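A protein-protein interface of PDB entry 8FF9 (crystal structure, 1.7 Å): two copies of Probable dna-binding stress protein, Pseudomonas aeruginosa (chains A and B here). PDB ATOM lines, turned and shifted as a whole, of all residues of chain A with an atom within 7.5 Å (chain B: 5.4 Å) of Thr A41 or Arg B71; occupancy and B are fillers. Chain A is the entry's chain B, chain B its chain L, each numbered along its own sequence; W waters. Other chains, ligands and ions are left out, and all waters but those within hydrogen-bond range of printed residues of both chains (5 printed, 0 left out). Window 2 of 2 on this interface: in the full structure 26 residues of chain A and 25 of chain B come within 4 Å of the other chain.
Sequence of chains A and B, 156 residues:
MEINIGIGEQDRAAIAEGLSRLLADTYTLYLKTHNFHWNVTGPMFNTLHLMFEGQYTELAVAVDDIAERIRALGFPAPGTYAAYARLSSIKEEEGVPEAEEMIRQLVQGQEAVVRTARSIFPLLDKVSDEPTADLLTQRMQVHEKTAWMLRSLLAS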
ATOM      1  N   ASN A  35      11.253  19.939 -11.854  1.00  0.00           N
ATOM      2  CA  ASN A  35      11.602  19.138 -10.690  1.00  0.00           C
ATOM      3  C   ASN A  35      12.131  17.773 -11.129  1.00  0.00           C
ATOM      4  O   ASN A  35      13.205  17.333 -10.703  1.00  0.00           O
ATOM      5  CB  ASN A  35      10.331  19.024  -9.823  1.00  0.00           C
ATOM      6  CG  ASN A  35      10.492  18.149  -8.593  1.00  0.00           C
ATOM      7  OD1 ASN A  35      11.187  17.129  -8.600  1.00  0.00           O
ATOM      8  ND2 ASN A  35       9.785  18.523  -7.525  1.00  0.00           N
ATOM      9  N   PHE A  36      11.380  17.093 -11.983  1.00  0.00           N
ATOM     10  CA  PHE A  36      11.784  15.752 -12.384  1.00  0.00           C
ATOM     11  C   PHE A  36      13.083  15.790 -13.201  1.00  0.00           C
ATOM     12  O   PHE A  36      13.892  14.857 -13.109  1.00  0.00           O
ATOM     13  CB  PHE A  36      10.662  15.075 -13.158  1.00  0.00           C
ATOM     14  CG  PHE A  36       9.446  14.685 -12.323  1.00  0.00           C
ATOM     15  CD1 PHE A  36       9.394  14.852 -10.941  1.00  0.00           C
ATOM     16  CD2 PHE A  36       8.348  14.134 -12.963  1.00  0.00           C
ATOM     17  CE1 PHE A  36       8.268  14.440 -10.223  1.00  0.00           C
ATOM     18  CE2 PHE A  36       7.243  13.742 -12.260  1.00  0.00           C
ATOM     19  CZ  PHE A  36       7.191  13.915 -10.888  1.00  0.00           C
ATOM     20  N   HIS A  37      13.297  16.849 -13.985  1.00  0.00           N
ATOM     21  CA  HIS A  37      14.559  17.049 -14.698  1.00  0.00           C
ATOM     22  C   HIS A  37      15.742  17.061 -13.732  1.00  0.00           C
ATOM     23  O   HIS A  37      16.741  16.374 -13.950  1.00  0.00           O
ATOM     24  CB  HIS A  37      14.468  18.349 -15.500  1.00  0.00           C
ATOM     25  CG  HIS A  37      15.787  18.930 -15.915  1.00  0.00           C
ATOM     26  ND1 HIS A  37      16.458  18.513 -17.046  1.00  0.00           N
ATOM     27  CD2 HIS A  37      16.500  19.962 -15.411  1.00  0.00           C
ATOM     28  CE1 HIS A  37      17.558  19.232 -17.187  1.00  0.00           C
ATOM     29  NE2 HIS A  37      17.601  20.125 -16.209  1.00  0.00           N
ATOM     30  N   TRP A  38      15.639  17.821 -12.639  1.00  0.00           N
ATOM     31  CA  TRP A  38      16.718  17.823 -11.671  1.00  0.00           C
ATOM     32  C   TRP A  38      16.891  16.474 -10.987  1.00  0.00           C
ATOM     33  O   TRP A  38      18.026  16.078 -10.680  1.00  0.00           O
ATOM     34  CB  TRP A  38      16.473  18.872 -10.599  1.00  0.00           C
ATOM     35  CG  TRP A  38      16.362  20.274 -11.073  1.00  0.00           C
ATOM     36  CD1 TRP A  38      17.065  20.878 -12.063  1.00  0.00           C
ATOM     37  CD2 TRP A  38      15.471  21.264 -10.546  1.00  0.00           C
ATOM     38  NE1 TRP A  38      16.675  22.197 -12.191  1.00  0.00           N
ATOM     39  CE2 TRP A  38      15.692  22.453 -11.270  1.00  0.00           C
ATOM     40  CE3 TRP A  38      14.517  21.257  -9.516  1.00  0.00           C
ATOM     41  CZ2 TRP A  38      14.999  23.626 -10.999  1.00  0.00           C
ATOM     42  CZ3 TRP A  38      13.816  22.431  -9.252  1.00  0.00           C
ATOM     43  CH2 TRP A  38      14.059  23.591  -9.998  1.00  0.00           C
ATOM     44  N   ASN A  39      15.782  15.808 -10.638  1.00  0.00           N
ATOM     45  CA  ASN A  39      15.813  14.762  -9.618  1.00  0.00           C
ATOM     46  C   ASN A  39      15.757  13.325 -10.136  1.00  0.00           C
ATOM     47  O   ASN A  39      15.955  12.394  -9.334  1.00  0.00           O
ATOM     48  CB  ASN A  39      14.658  14.990  -8.641  1.00  0.00           C
ATOM     49  CG  ASN A  39      14.925  16.170  -7.729  1.00  0.00           C
ATOM     50  OD1 ASN A  39      15.891  16.153  -6.984  1.00  0.00           O
ATOM     51  ND2 ASN A  39      14.092  17.211  -7.803  1.00  0.00           N
ATOM     52  N   VAL A  40      15.500  13.118 -11.430  1.00  0.00           N
ATOM     53  CA  VAL A  40      15.419  11.771 -11.986  1.00  0.00           C
ATOM     54  C   VAL A  40      16.758  11.059 -11.818  1.00  0.00           C
ATOM     55  O   VAL A  40      17.827  11.675 -11.948  1.00  0.00           O
ATOM     56  CB  VAL A  40      14.981  11.828 -13.460  1.00  0.00           C
ATOM     57  CG1 VAL A  40      15.983  12.568 -14.353  1.00  0.00           C
ATOM     58  CG2 VAL A  40      14.693  10.432 -14.005  1.00  0.00           C
ATOM     59  N   THR A  41      16.708   9.752 -11.533  1.00  0.00           N
ATOM     60  CA  THR A  41      17.927   8.934 -11.498  1.00  0.00           C
ATOM     61  C   THR A  41      17.661   7.565 -12.114  1.00  0.00           C
ATOM     62  O   THR A  41      16.534   7.227 -12.480  1.00  0.00           O
ATOM     63  CB  THR A  41      18.469   8.743 -10.075  1.00  0.00           C
ATOM     64  OG1 THR A  41      17.519   8.023  -9.291  1.00  0.00           O
ATOM     65  CG2 THR A  41      18.813  10.092  -9.394  1.00  0.00           C
ATOM     66  N   GLY A  42      18.724   6.762 -12.210  1.00  0.00           N
ATOM     67  CA  GLY A  42      18.647   5.475 -12.858  1.00  0.00           C
ATOM     68  C   GLY A  42      19.259   5.465 -14.240  1.00  0.00           C
ATOM     69  O   GLY A  42      19.752   6.483 -14.745  1.00  0.00           O
ATOM     70  N   PRO A  43      19.205   4.307 -14.899  1.00  0.00           N
ATOM     71  CA  PRO A  43      19.856   4.172 -16.213  1.00  0.00           C
ATOM     72  C   PRO A  43      19.262   5.056 -17.290  1.00  0.00           C
ATOM     73  O   PRO A  43      19.918   5.285 -18.314  1.00  0.00           O
ATOM     74  CB  PRO A  43      19.677   2.680 -16.547  1.00  0.00           C
ATOM     75  CG  PRO A  43      19.416   2.014 -15.257  1.00  0.00           C
ATOM     76  CD  PRO A  43      18.683   3.023 -14.401  1.00  0.00           C
ATOM     77  N   MET A  44      18.050   5.574 -17.096  1.00  0.00           N
ATOM     78  CA  MET A  44      17.460   6.488 -18.058  1.00  0.00           C
ATOM     79  C   MET A  44      17.789   7.939 -17.748  1.00  0.00           C
ATOM     80  O   MET A  44      17.247   8.838 -18.405  1.00  0.00           O
ATOM     81  CB  MET A  44      15.944   6.279 -18.097  1.00  0.00           C
ATOM     82  CG  MET A  44      15.522   4.849 -18.492  1.00  0.00           C
ATOM     83  SD  MET A  44      13.741   4.641 -18.287  1.00  0.00           S
ATOM     84  CE  MET A  44      13.288   5.417 -19.822  1.00  0.00           C
ATOM     85  N   PHE A  45      18.715   8.186 -16.808  1.00  0.00           N
ATOM     86  CA  PHE A  45      19.023   9.562 -16.408  1.00  0.00           C
ATOM     87  C   PHE A  45      19.306  10.480 -17.595  1.00  0.00           C
ATOM     88  O   PHE A  45      18.740  11.572 -17.678  1.00  0.00           O
ATOM     89  CB  PHE A  45      20.215   9.636 -15.460  1.00  0.00           C
ATOM     90  CG  PHE A  45      20.664  11.062 -15.226  1.00  0.00           C
ATOM     91  CD1 PHE A  45      19.947  11.873 -14.363  1.00  0.00           C
ATOM     92  CD2 PHE A  45      21.746  11.606 -15.915  1.00  0.00           C
ATOM     93  CE1 PHE A  45      20.318  13.192 -14.147  1.00  0.00           C
ATOM     94  CE2 PHE A  45      22.120  12.929 -15.734  1.00  0.00           C
ATOM     95  CZ  PHE A  45      21.407  13.732 -14.853  1.00  0.00           C
ATOM     96  N   ASN A  46      20.234  10.113 -18.485  1.00  0.00           N
ATOM     97  CA  ASN A  46      20.647  11.070 -19.508  1.00  0.00           C
ATOM     98  C   ASN A  46      19.484  11.437 -20.421  1.00  0.00           C
ATOM     99  O   ASN A  46      19.249  12.618 -20.710  1.00  0.00           O
ATOM    100  CB  ASN A  46      21.776  10.513 -20.366  1.00  0.00           C
ATOM    101  CG  ASN A  46      23.117  10.548 -19.676  1.00  0.00           C
ATOM    102  OD1 ASN A  46      23.434  11.483 -18.943  1.00  0.00           O
ATOM    103  ND2 ASN A  46      23.927   9.536 -19.937  1.00  0.00           N
ATOM    104  N   LEU A  48      16.149  11.043 -19.962  1.00  0.00           N
ATOM    105  CA  LEU A  48      15.029  11.730 -19.314  1.00  0.00           C
ATOM    106  C   LEU A  48      15.418  13.133 -18.849  1.00  0.00           C
ATOM    107  O   LEU A  48      14.599  14.055 -18.912  1.00  0.00           O
ATOM    108  CB  LEU A  48      14.487  10.912 -18.136  1.00  0.00           C
ATOM    109  CG  LEU A  48      13.867   9.556 -18.467  1.00  0.00           C
ATOM    110  CD1 LEU A  48      13.451   8.854 -17.210  1.00  0.00           C
ATOM    111  CD2 LEU A  48      12.706   9.756 -19.436  1.00  0.00           C
ATOM    112  N   HIS A  49      16.649  13.326 -18.366  1.00  0.00           N
ATOM    113  CA  HIS A  49      17.117  14.676 -18.055  1.00  0.00           C
ATOM    114  C   HIS A  49      16.946  15.580 -19.265  1.00  0.00           C
ATOM    115  O   HIS A  49      16.360  16.665 -19.170  1.00  0.00           O
ATOM    116  CB  HIS A  49      18.581  14.587 -17.597  1.00  0.00           C
ATOM    117  CG  HIS A  49      19.176  15.845 -17.047  1.00  0.00           C
ATOM    118  ND1 HIS A  49      18.800  16.390 -15.837  1.00  0.00           N
ATOM    119  CD2 HIS A  49      20.209  16.604 -17.494  1.00  0.00           C
ATOM    120  CE1 HIS A  49      19.551  17.440 -15.576  1.00  0.00           C
ATOM    121  NE2 HIS A  49      20.411  17.597 -16.565  1.00  0.00           N
ATOM    122  N   VAL A  96      10.495  12.045  -4.449  1.00  0.00           N
ATOM    123  CA  VAL A  96      11.329  11.721  -5.603  1.00  0.00           C
ATOM    124  C   VAL A  96      10.939  10.325  -6.077  1.00  0.00           C
ATOM    125  O   VAL A  96      11.497   9.317  -5.605  1.00  0.00           O
ATOM    126  CB  VAL A  96      12.825  11.786  -5.273  1.00  0.00           C
ATOM    127  CG1 VAL A  96      13.631  11.567  -6.541  1.00  0.00           C
ATOM    128  CG2 VAL A  96      13.209  13.105  -4.650  1.00  0.00           C
ATOM    129  N   PRO A  97       9.983  10.208  -6.985  1.00  0.00           N
ATOM    130  CA  PRO A  97       9.605   8.887  -7.484  1.00  0.00           C
ATOM    131  C   PRO A  97      10.685   8.258  -8.343  1.00  0.00           C
ATOM    132  O   PRO A  97      11.624   8.907  -8.804  1.00  0.00           O
ATOM    133  CB  PRO A  97       8.341   9.162  -8.313  1.00  0.00           C
ATOM    134  CG  PRO A  97       7.889  10.533  -7.917  1.00  0.00           C
ATOM    135  CD  PRO A  97       9.106  11.269  -7.508  1.00  0.00           C
ATOM    136  N   GLU A  98      10.532   6.948  -8.554  1.00  0.00           N
ATOM    137  CA  GLU A  98      11.336   6.260  -9.550  1.00  0.00           C
ATOM    138  C   GLU A  98      11.013   6.807 -10.943  1.00  0.00           C
ATOM    139  O   GLU A  98       9.934   7.355 -11.193  1.00  0.00           O
ATOM    140  CB  GLU A  98      11.092   4.748  -9.492  1.00  0.00           C
ATOM    141  CG  GLU A  98      11.612   4.075  -8.203  1.00  0.00           C
ATOM    142  N   ALA A  99      11.967   6.641 -11.861  1.00  0.00           N
ATOM    143  CA  ALA A  99      11.851   7.260 -13.178  1.00  0.00           C
ATOM    144  C   ALA A  99      10.563   6.876 -13.881  1.00  0.00           C
ATOM    145  O   ALA A  99       9.929   7.708 -14.538  1.00  0.00           O
ATOM    146  CB  ALA A  99      13.042   6.871 -14.039  1.00  0.00           C
ATOM    147  N   GLU A 100      10.180   5.610 -13.796  1.00  0.00           N
ATOM    148  CA  GLU A 100       8.976   5.173 -14.500  1.00  0.00           C
ATOM    149  C   GLU A 100       7.709   5.828 -13.941  1.00  0.00           C
ATOM    150  O   GLU A 100       6.766   6.078 -14.701  1.00  0.00           O
ATOM    151  CB  GLU A 100       8.864   3.646 -14.444  1.00  0.00           C
ATOM    152  CG  GLU A 100       9.967   2.914 -15.201  1.00  0.00           C
ATOM    153  CD  GLU A 100      11.318   2.816 -14.442  1.00  0.00           C
ATOM    154  OE1 GLU A 100      11.433   3.199 -13.240  1.00  0.00           O
ATOM    155  OE2 GLU A 100      12.280   2.329 -15.077  1.00  0.00           O
ATOM    156  N   MET A 102       7.776   8.881 -12.486  1.00  0.00           N
ATOM    157  CA  MET A 102       7.867  10.240 -13.010  1.00  0.00           C
ATOM    158  C   MET A 102       7.255  10.326 -14.398  1.00  0.00           C
ATOM    159  O   MET A 102       6.498  11.251 -14.693  1.00  0.00           O
ATOM    160  CB  MET A 102       9.315  10.699 -13.062  1.00  0.00           C
ATOM    161  CG  MET A 102       9.922  11.021 -11.720  1.00  0.00           C
ATOM    162  SD  MET A 102      11.631  11.566 -11.898  1.00  0.00           S
ATOM    163  CE  MET A 102      11.934  12.021 -10.189  1.00  0.00           C
ATOM    164  N   ILE B  66      21.434  26.504  -9.264  1.00  0.00           N
ATOM    165  CA  ILE B  66      21.348  26.227  -7.827  1.00  0.00           C
ATOM    166  C   ILE B  66      20.880  24.795  -7.591  1.00  0.00           C
ATOM    167  O   ILE B  66      21.457  24.060  -6.778  1.00  0.00           O
ATOM    168  CB  ILE B  66      20.425  27.252  -7.134  1.00  0.00           C
ATOM    169  CG1 ILE B  66      20.944  28.686  -7.323  1.00  0.00           C
ATOM    170  CG2 ILE B  66      20.264  26.878  -5.649  1.00  0.00           C
ATOM    171  CD1 ILE B  66      19.881  29.761  -7.027  1.00  0.00           C
ATOM    172  N   ALA B  67      19.841  24.369  -8.317  1.00  0.00           N
ATOM    173  CA  ALA B  67      19.342  23.005  -8.174  1.00  0.00           C
ATOM    174  C   ALA B  67      20.429  21.982  -8.486  1.00  0.00           C
ATOM    175  O   ALA B  67      20.551  20.962  -7.793  1.00  0.00           O
ATOM    176  CB  ALA B  67      18.134  22.801  -9.088  1.00  0.00           C
ATOM    177  N   GLU B  68      21.223  22.229  -9.520  1.00  0.00           N
ATOM    178  CA  GLU B  68      22.268  21.268  -9.881  1.00  0.00           C
ATOM    179  C   GLU B  68      23.339  21.165  -8.807  1.00  0.00           C
ATOM    180  O   GLU B  68      23.941  20.098  -8.641  1.00  0.00           O
ATOM    181  CB  GLU B  68      22.922  21.644 -11.205  1.00  0.00           C
ATOM    182  CG  GLU B  68      22.048  21.321 -12.374  1.00  0.00           C
ATOM    183  CD  GLU B  68      22.645  21.761 -13.696  1.00  0.00           C
ATOM    184  OE1 GLU B  68      23.780  22.342 -13.733  1.00  0.00           O
ATOM    185  OE2 GLU B  68      21.957  21.513 -14.699  1.00  0.00           O
ATOM    186  N   ARG B  69      23.630  22.265  -8.103  1.00  0.00           N
ATOM    187  CA  ARG B  69      24.606  22.176  -7.021  1.00  0.00           C
ATOM    188  C   ARG B  69      24.064  21.334  -5.870  1.00  0.00           C
ATOM    189  O   ARG B  69      24.800  20.548  -5.263  1.00  0.00           O
ATOM    190  CB  ARG B  69      25.000  23.579  -6.545  1.00  0.00           C
ATOM    191  CG  ARG B  69      26.134  23.579  -5.464  1.00  0.00           C
ATOM    192  CD  ARG B  69      27.425  22.912  -5.979  1.00  0.00           C
ATOM    193  NE  ARG B  69      28.427  22.715  -4.934  1.00  0.00           N
ATOM    194  CZ  ARG B  69      29.403  21.829  -5.019  1.00  0.00           C
ATOM    195  NH1 ARG B  69      29.555  21.081  -6.101  1.00  0.00           N
ATOM    196  NH2 ARG B  69      30.235  21.677  -3.987  1.00  0.00           N
ATOM    197  N   ILE B  70      22.774  21.471  -5.566  1.00  0.00           N
ATOM    198  CA  ILE B  70      22.150  20.622  -4.558  1.00  0.00           C
ATOM    199  C   ILE B  70      22.291  19.165  -4.955  1.00  0.00           C
ATOM    200  O   ILE B  70      22.610  18.307  -4.121  1.00  0.00           O
ATOM    201  CB  ILE B  70      20.669  21.015  -4.367  1.00  0.00           C
ATOM    202  CG1 ILE B  70      20.559  22.414  -3.741  1.00  0.00           C
ATOM    203  CG2 ILE B  70      19.918  20.028  -3.496  1.00  0.00           C
ATOM    204  CD1 ILE B  70      19.143  23.011  -3.776  1.00  0.00           C
ATOM    205  N   ARG B  71      22.044  18.860  -6.239  1.00  0.00           N
ATOM    206  CA  ARG B  71      22.184  17.481  -6.709  1.00  0.00           C
ATOM    207  C   ARG B  71      23.627  17.011  -6.603  1.00  0.00           C
ATOM    208  O   ARG B  71      23.886  15.867  -6.210  1.00  0.00           O
ATOM    209  CB  ARG B  71      21.691  17.352  -8.148  1.00  0.00           C
ATOM    210  CG  ARG B  71      20.206  17.694  -8.333  1.00  0.00           C
ATOM    211  CD  ARG B  71      19.248  16.733  -7.634  1.00  0.00           C
ATOM    212  NE  ARG B  71      19.383  15.356  -8.096  1.00  0.00           N
ATOM    213  CZ  ARG B  71      19.835  14.346  -7.360  1.00  0.00           C
ATOM    214  NH1 ARG B  71      20.178  14.505  -6.087  1.00  0.00           N
ATOM    215  NH2 ARG B  71      19.942  13.143  -7.909  1.00  0.00           N
ATOM    216  N   ALA B  72      24.582  17.872  -6.945  1.00  0.00           N
ATOM    217  CA  ALA B  72      25.986  17.484  -6.831  1.00  0.00           C
ATOM    218  C   ALA B  72      26.343  17.153  -5.385  1.00  0.00           C
ATOM    219  O   ALA B  72      27.230  16.328  -5.121  1.00  0.00           O
ATOM    220  CB  ALA B  72      26.875  18.605  -7.386  1.00  0.00           C
ATOM    221  N   LEU B  73      25.649  17.762  -4.438  1.00  0.00           N
ATOM    222  CA  LEU B  73      25.912  17.513  -3.033  1.00  0.00           C
ATOM    223  C   LEU B  73      25.193  16.265  -2.538  1.00  0.00           C
ATOM    224  O   LEU B  73      25.378  15.882  -1.384  1.00  0.00           O
ATOM    225  CB  LEU B  73      25.508  18.725  -2.192  1.00  0.00           C
ATOM    226  CG  LEU B  73      26.399  19.952  -2.331  1.00  0.00           C
ATOM    227  CD1 LEU B  73      25.716  21.172  -1.693  1.00  0.00           C
ATOM    228  CD2 LEU B  73      27.764  19.718  -1.692  1.00  0.00           C
ATOM    229  N   GLY B  74      24.383  15.634  -3.382  1.00  0.00           N
ATOM    230  CA  GLY B  74      23.749  14.383  -3.043  1.00  0.00           C
ATOM    231  C   GLY B  74      22.385  14.503  -2.423  1.00  0.00           C
ATOM    232  O   GLY B  74      21.963  13.581  -1.706  1.00  0.00           O
ATOM    233  N   PHE B  75      21.670  15.596  -2.678  1.00  0.00           N
ATOM    234  CA  PHE B  75      20.347  15.810  -2.108  1.00  0.00           C
ATOM    235  C   PHE B  75      19.346  16.164  -3.190  1.00  0.00           C
ATOM    236  O   PHE B  75      19.706  16.704  -4.242  1.00  0.00           O
ATOM    237  CB  PHE B  75      20.386  16.897  -1.030  1.00  0.00           C
ATOM    238  CG  PHE B  75      21.075  16.407   0.191  1.00  0.00           C
ATOM    239  CD1 PHE B  75      22.453  16.445   0.283  1.00  0.00           C
ATOM    240  CD2 PHE B  75      20.366  15.730   1.140  1.00  0.00           C
ATOM    241  CE1 PHE B  75      23.098  15.888   1.363  1.00  0.00           C
ATOM    242  CE2 PHE B  75      21.013  15.177   2.230  1.00  0.00           C
ATOM    243  CZ  PHE B  75      22.381  15.258   2.327  1.00  0.00           C
ATOM    244  N   PRO B  76      18.085  15.823  -2.976  1.00  0.00           N
ATOM    245  CA  PRO B  76      17.069  16.203  -3.956  1.00  0.00           C
ATOM    246  C   PRO B  76      16.842  17.705  -3.932  1.00  0.00           C
ATOM    247  O   PRO B  76      16.927  18.369  -2.888  1.00  0.00           O
ATOM    248  CB  PRO B  76      15.830  15.418  -3.516  1.00  0.00           C
ATOM    249  CG  PRO B  76      16.005  15.184  -2.047  1.00  0.00           C
ATOM    250  CD  PRO B  76      17.517  15.136  -1.804  1.00  0.00           C
ATOM    251  N   ALA B  77      16.586  18.243  -5.107  1.00  0.00           N
ATOM    252  CA  ALA B  77      16.277  19.658  -5.238  1.00  0.00           C
ATOM    253  C   ALA B  77      14.784  19.855  -5.028  1.00  0.00           C
ATOM    254  O   ALA B  77      13.988  19.219  -5.727  1.00  0.00           O
ATOM    255  CB  ALA B  77      16.666  20.155  -6.619  1.00  0.00           C
HETATM  256  O   HOH W   1      12.665  16.849  -4.829  1.00  0.00           O
HETATM  257  O   HOH W   2      16.843  13.536  -6.639  1.00  0.00           O
HETATM  258  O   HOH W   3      22.373  19.496 -16.505  1.00  0.00           O
HETATM  259  O   HOH W   4      19.801  20.250 -14.213  1.00  0.00           O
HETATM  260  O   HOH W   5      19.176  13.629 -10.742  1.00  0.00           O
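O of Trp A38 is in hydrogen-bond range of NE of Arg B71, at 3.0 Å. The side-chain amide nitrogen (ND2) of Asn A39 sits at hydrogen-bond distance from the backbone carbonyl oxygen (O) of Ala B77 (2.9 Å).
OD1 of Asn A35 sits at hydrogen-bond distance from ND2 of Asn A39 (3.0 Å). NH1 of Arg B71 sits at hydrogen-bond distance from O of Phe B75, at 2.9 Å.
Among the printed residues, merely in contact across the chains: Trp A38 with Ala B67 (3.3 Å), Trp A38 with Ala B77 (3.8 Å), Asn A39 with Arg B71 (3.5 Å), Asn A39 with Pro B76 (3.2 Å), Thr A41 with Arg B71 (3.6 Å) and Val A96 with Pro B76 (3.7 Å).
Of the printed residues of chain B, Asn A39 touches Arg B71 (3.5 Å), Pro B76 (3.2 Å) and Ala B77 (2.9 Å). Printed residues of chain A within 4 Å of Ala B67: Trp A38 (3.3 Å). Arg B69 touches none of the printed residues of chain A. Printed residues of chain A within 4 Å of Arg B71: Trp A38, Asn A39 and Thr A41. Gly B74 touches none of the printed residues of chain A. The nearest residue of chain A that does not touch Arg B71 is Val A40 (4.8 Å). The nearest printed residue of chain B that does not touch Trp A38 is Glu B68 (5.0 Å).
Hydrophobic or aromatic side chains of chain B that line the printed part of chain A: Ala B67, Pro B76 and Ala B77. Among the printed residues, 8 pairs touch across the chains. Among the printed residues, no Asp or Glu carboxylate lies within 4 Å of a Lys or Arg side-chain nitrogen of the other chain.
No position is printed for both chains. Of the 8 pairs that touch across the chains among the printed residues, none has its exchanged pair printed and touching as well.
Water W4 bridges the side-chain carboxylate of Glu B68 and a ring nitrogen (NE2) of His A37. Water W5 lies within hydrogen-bond range of O of Val A40 (2.7 Å), O of Trp A38 (2.7 Å) and NH2 of Arg B71 (3.0 Å). Water W3 bridges a ring nitrogen (NE2) of His A49 and the side-chain carboxylate (OE2) of Glu B68. Water W2 lies within hydrogen-bond range of OD1 of Asn A39 and NH2 of Arg B71. Water W1 lies within hydrogen-bond range of O of Ala B77 (2.9 Å) and ND2 of Asn A39 (3.3 Å).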
